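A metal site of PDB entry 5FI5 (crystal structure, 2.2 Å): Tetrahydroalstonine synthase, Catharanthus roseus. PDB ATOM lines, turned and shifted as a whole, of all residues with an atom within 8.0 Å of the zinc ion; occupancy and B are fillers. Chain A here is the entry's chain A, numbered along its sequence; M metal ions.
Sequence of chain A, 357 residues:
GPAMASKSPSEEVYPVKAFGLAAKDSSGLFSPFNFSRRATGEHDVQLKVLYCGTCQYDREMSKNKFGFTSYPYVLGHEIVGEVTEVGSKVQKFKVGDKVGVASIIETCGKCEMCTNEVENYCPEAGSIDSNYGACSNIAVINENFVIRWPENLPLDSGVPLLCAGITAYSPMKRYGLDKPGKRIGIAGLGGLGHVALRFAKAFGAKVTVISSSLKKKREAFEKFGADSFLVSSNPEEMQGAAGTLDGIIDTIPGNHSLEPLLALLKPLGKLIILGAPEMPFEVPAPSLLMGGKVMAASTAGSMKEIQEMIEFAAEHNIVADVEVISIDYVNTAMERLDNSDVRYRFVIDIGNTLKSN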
ATOM      1  N   GLY A  53      33.617 -17.936   9.447  1.00  0.00           N
ATOM      2  CA  GLY A  53      32.574 -18.950   9.509  1.00  0.00           C
ATOM      3  C   GLY A  53      32.818 -19.948   8.408  1.00  0.00           C
ATOM      4  O   GLY A  53      33.323 -19.603   7.346  1.00  0.00           O
ATOM      5  N   THR A  54      32.421 -21.174   8.652  1.00  0.00           N
ATOM      6  CA  THR A  54      32.779 -22.309   7.800  1.00  0.00           C
ATOM      7  C   THR A  54      31.520 -23.157   7.566  1.00  0.00           C
ATOM      8  O   THR A  54      30.634 -23.186   8.430  1.00  0.00           O
ATOM      9  CB  THR A  54      33.947 -23.085   8.483  1.00  0.00           C
ATOM     10  OG1 THR A  54      34.968 -23.391   7.547  1.00  0.00           O
ATOM     11  CG2 THR A  54      33.517 -24.350   9.173  1.00  0.00           C
ATOM     12  N   CYS A  55      31.452 -23.860   6.436  1.00  0.00           N
ATOM     13  CA  CYS A  55      30.331 -24.795   6.166  1.00  0.00           C
ATOM     14  C   CYS A  55      30.647 -25.864   5.087  1.00  0.00           C
ATOM     15  O   CYS A  55      31.790 -25.988   4.640  1.00  0.00           O
ATOM     16  CB  CYS A  55      29.082 -23.999   5.775  1.00  0.00           C
ATOM     17  SG  CYS A  55      29.165 -23.320   4.109  1.00  0.00           S
ATOM     18  N   GLN A  56      29.616 -26.595   4.659  1.00  0.00           N
ATOM     19  CA  GLN A  56      29.724 -27.649   3.655  1.00  0.00           C
ATOM     20  C   GLN A  56      30.432 -27.188   2.382  1.00  0.00           C
ATOM     21  O   GLN A  56      31.292 -27.895   1.887  1.00  0.00           O
ATOM     22  CB  GLN A  56      28.319 -28.182   3.312  1.00  0.00           C
ATOM     23  CG  GLN A  56      28.249 -29.412   2.417  1.00  0.00           C
ATOM     24  CD  GLN A  56      28.916 -30.696   2.954  1.00  0.00           C
ATOM     25  OE1 GLN A  56      29.329 -31.569   2.173  1.00  0.00           O
ATOM     26  NE2 GLN A  56      28.999 -30.826   4.265  1.00  0.00           N
ATOM     27  N   TYR A  57      30.086 -25.993   1.888  1.00  0.00           N
ATOM     28  CA  TYR A  57      30.724 -25.402   0.689  1.00  0.00           C
ATOM     29  C   TYR A  57      32.258 -25.462   0.735  1.00  0.00           C
ATOM     30  O   TYR A  57      32.883 -25.808  -0.247  1.00  0.00           O
ATOM     31  CB  TYR A  57      30.246 -23.952   0.478  1.00  0.00           C
ATOM     32  CG  TYR A  57      30.890 -23.118  -0.634  1.00  0.00           C
ATOM     33  CD1 TYR A  57      31.966 -22.253  -0.351  1.00  0.00           C
ATOM     34  CD2 TYR A  57      30.385 -23.138  -1.941  1.00  0.00           C
ATOM     35  CE1 TYR A  57      32.532 -21.450  -1.340  1.00  0.00           C
ATOM     36  CE2 TYR A  57      30.955 -22.341  -2.943  1.00  0.00           C
ATOM     37  CZ  TYR A  57      32.019 -21.493  -2.640  1.00  0.00           C
ATOM     38  OH  TYR A  57      32.599 -20.691  -3.632  1.00  0.00           O
ATOM     39  N   ASP A  58      32.839 -25.158   1.894  1.00  0.00           N
ATOM     40  CA  ASP A  58      34.299 -25.192   2.064  1.00  0.00           C
ATOM     41  C   ASP A  58      34.879 -26.593   1.881  1.00  0.00           C
ATOM     42  O   ASP A  58      35.904 -26.746   1.221  1.00  0.00           O
ATOM     43  CB  ASP A  58      34.703 -24.705   3.455  1.00  0.00           C
ATOM     44  CG  ASP A  58      34.433 -23.241   3.687  1.00  0.00           C
ATOM     45  OD1 ASP A  58      34.835 -22.396   2.864  1.00  0.00           O
ATOM     46  OD2 ASP A  58      33.836 -22.943   4.747  1.00  0.00           O
ATOM     47  N   GLY A  76      37.514 -19.815   2.867  1.00  0.00           N
ATOM     48  CA  GLY A  76      37.035 -18.707   3.705  1.00  0.00           C
ATOM     49  C   GLY A  76      36.032 -17.800   3.000  1.00  0.00           C
ATOM     50  O   GLY A  76      36.424 -16.866   2.314  1.00  0.00           O
ATOM     51  N   HIS A  77      34.735 -18.055   3.222  1.00  0.00           N
ATOM     52  CA  HIS A  77      33.652 -17.286   2.595  1.00  0.00           C
ATOM     53  C   HIS A  77      32.651 -16.583   3.534  1.00  0.00           C
ATOM     54  O   HIS A  77      31.743 -15.930   3.055  1.00  0.00           O
ATOM     55  CB  HIS A  77      32.898 -18.180   1.606  1.00  0.00           C
ATOM     56  CG  HIS A  77      32.087 -19.253   2.246  1.00  0.00           C
ATOM     57  ND1 HIS A  77      32.640 -20.448   2.659  1.00  0.00           N
ATOM     58  CD2 HIS A  77      30.777 -19.319   2.546  1.00  0.00           C
ATOM     59  CE1 HIS A  77      31.692 -21.199   3.191  1.00  0.00           C
ATOM     60  NE2 HIS A  77      30.556 -20.538   3.144  1.00  0.00           N
ATOM     61  N   GLU A  78      32.798 -16.742   4.847  1.00  0.00           N
ATOM     62  CA  GLU A  78      31.936 -16.095   5.840  1.00  0.00           C
ATOM     63  C   GLU A  78      32.874 -15.375   6.796  1.00  0.00           C
ATOM     64  O   GLU A  78      33.520 -16.010   7.642  1.00  0.00           O
ATOM     65  CB  GLU A  78      31.061 -17.122   6.608  1.00  0.00           C
ATOM     66  CG  GLU A  78      30.565 -18.341   5.818  1.00  0.00           C
ATOM     67  CD  GLU A  78      29.808 -19.352   6.692  1.00  0.00           C
ATOM     68  OE1 GLU A  78      29.676 -19.097   7.914  1.00  0.00           O
ATOM     69  OE2 GLU A  78      29.350 -20.413   6.171  1.00  0.00           O
ATOM     70  N   SER A 103      30.101 -14.447   0.517  1.00  0.00           N
ATOM     71  CA  SER A 103      30.695 -15.287  -0.552  1.00  0.00           C
ATOM     72  C   SER A 103      31.043 -14.504  -1.818  1.00  0.00           C
ATOM     73  O   SER A 103      32.128 -14.668  -2.357  1.00  0.00           O
ATOM     74  CB  SER A 103      29.742 -16.441  -0.916  1.00  0.00           C
ATOM     75  OG  SER A 103      28.410 -15.983  -1.274  1.00  0.00           O
ATOM     76  N   VAL A 159      28.781 -14.325  12.575  1.00  0.00           N
ATOM     77  CA  VAL A 159      29.375 -14.509  11.249  1.00  0.00           C
ATOM     78  C   VAL A 159      28.641 -15.490  10.320  1.00  0.00           C
ATOM     79  O   VAL A 159      28.507 -15.205   9.127  1.00  0.00           O
ATOM     80  CB  VAL A 159      30.919 -14.708  11.292  1.00  0.00           C
ATOM     81  CG1 VAL A 159      31.327 -16.057  11.896  1.00  0.00           C
ATOM     82  CG2 VAL A 159      31.545 -14.555   9.902  1.00  0.00           C
ATOM     83  N   PRO A 160      28.106 -16.628  10.840  1.00  0.00           N
ATOM     84  CA  PRO A 160      27.356 -17.479   9.891  1.00  0.00           C
ATOM     85  C   PRO A 160      26.070 -16.890   9.293  1.00  0.00           C
ATOM     86  O   PRO A 160      25.554 -17.428   8.319  1.00  0.00           O
ATOM     87  CB  PRO A 160      27.008 -18.732  10.725  1.00  0.00           C
ATOM     88  CG  PRO A 160      28.023 -18.746  11.811  1.00  0.00           C
ATOM     89  CD  PRO A 160      28.199 -17.284  12.165  1.00  0.00           C
ATOM     90  N   LEU A 162      25.990 -14.483   7.512  1.00  0.00           N
ATOM     91  CA  LEU A 162      26.415 -14.058   6.181  1.00  0.00           C
ATOM     92  C   LEU A 162      26.306 -15.164   5.092  1.00  0.00           C
ATOM     93  O   LEU A 162      26.455 -14.861   3.901  1.00  0.00           O
ATOM     94  CB  LEU A 162      27.853 -13.518   6.227  1.00  0.00           C
ATOM     95  CG  LEU A 162      28.064 -12.270   7.099  1.00  0.00           C
ATOM     96  CD1 LEU A 162      29.537 -11.945   7.214  1.00  0.00           C
ATOM     97  CD2 LEU A 162      27.308 -11.066   6.540  1.00  0.00           C
ATOM     98  N   CYS A 163      26.095 -16.410   5.504  1.00  0.00           N
ATOM     99  CA  CYS A 163      25.919 -17.528   4.582  1.00  0.00           C
ATOM    100  C   CYS A 163      24.509 -18.086   4.851  1.00  0.00           C
ATOM    101  O   CYS A 163      23.596 -17.881   4.051  1.00  0.00           O
ATOM    102  CB  CYS A 163      27.041 -18.532   4.814  1.00  0.00           C
ATOM    103  SG  CYS A 163      27.044 -20.070   3.855  1.00  0.00           S
ATOM    104  N   ALA A 164      24.311 -18.736   5.992  1.00  0.00           N
ATOM    105  CA  ALA A 164      23.038 -19.380   6.320  1.00  0.00           C
ATOM    106  C   ALA A 164      21.892 -18.393   6.496  1.00  0.00           C
ATOM    107  O   ALA A 164      20.748 -18.677   6.108  1.00  0.00           O
ATOM    108  CB  ALA A 164      23.184 -20.225   7.580  1.00  0.00           C
ATOM    109  N   THR A 167      20.878 -16.806   3.120  1.00  0.00           N
ATOM    110  CA  THR A 167      20.253 -17.869   2.318  1.00  0.00           C
ATOM    111  C   THR A 167      18.770 -18.072   2.671  1.00  0.00           C
ATOM    112  O   THR A 167      17.928 -18.266   1.787  1.00  0.00           O
ATOM    113  CB  THR A 167      21.027 -19.174   2.443  1.00  0.00           C
ATOM    114  OG1 THR A 167      22.357 -18.975   1.982  1.00  0.00           O
ATOM    115  CG2 THR A 167      20.388 -20.283   1.622  1.00  0.00           C
ATOM    116  N   ARG A 345      27.329 -24.630  13.652  1.00  0.00           N
ATOM    117  CA  ARG A 345      28.448 -24.272  12.787  1.00  0.00           C
ATOM    118  C   ARG A 345      29.876 -24.048  13.378  1.00  0.00           C
ATOM    119  O   ARG A 345      30.058 -23.390  14.413  1.00  0.00           O
ATOM    120  CB  ARG A 345      28.116 -22.984  12.083  1.00  0.00           C
ATOM    121  CG  ARG A 345      26.645 -22.733  11.818  1.00  0.00           C
ATOM    122  CD  ARG A 345      26.235 -23.275  10.488  1.00  0.00           C
ATOM    123  NE  ARG A 345      26.758 -22.467   9.393  1.00  0.00           N
ATOM    124  CZ  ARG A 345      26.276 -22.453   8.153  1.00  0.00           C
ATOM    125  NH1 ARG A 345      25.232 -23.216   7.814  1.00  0.00           N
ATOM    126  NH2 ARG A 345      26.830 -21.666   7.246  1.00  0.00           N
HETATM  127 ZN    ZN M   1      29.073 -20.974   4.269  1.00  0.00          ZN
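Arg 345 touches the zinc ion (NH2 to ZN, 3.8 Å).
Five residues have an atom within 4 Å of the zinc ion: Cys 55, His 77, Glu 78, Cys 163 and Arg 345.
Along chain A the residues within 4 Å of the zinc ion span positions 55 to 345.
The nearest printed residue that does not touch the zinc ion is Thr 54 (4.7 Å).
The zinc ion is bound by a ring nitrogen (NE2) of His 77 (1.9 Å).
The zinc ion is bound by OE2 of Glu 78, 2.0 Å away.
The side-chain sulfur (SG) of Cys 163 is bound to the zinc ion, at 2.3 Å.
The zinc ion is bound by SG of Cys 55 (2.4 Å).
The zinc ion has four donor atoms within binding distance.
The backbone carbonyl oxygen (O) of Glu 78 is in hydrogen-bond range of the backbone NH (N) of Gly 53.
The backbone NH of Tyr 57 lies close to the side-chain sulfur of Cys 55 (3.6 Å).
N of Cys 55 is in hydrogen-bond range of OD2 of Asp 58, at 3.1 Å.
The side-chain sulfur (SG) of Cys 163 sits close to the guanidinium group (NH2) of Arg 345 (3.8 Å).
NH2 of Arg 345 is in salt-bridge range of OE1 of Glu 78, at 3.9 Å.
A ring nitrogen (ND1) of His 77 lies within hydrogen-bond range of the side-chain carboxylate (OD1) of Asp 58, 2.9 Å away.
The backbone carbonyl oxygen (O) of Cys 163 lies within hydrogen-bond range of the side-chain hydroxyl (OG1) of Thr 167 (2.6 Å).
The backbone NH (N) of Ser 103 lies within hydrogen-bond range of the backbone carbonyl oxygen (O) of His 77 (3.4 Å).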
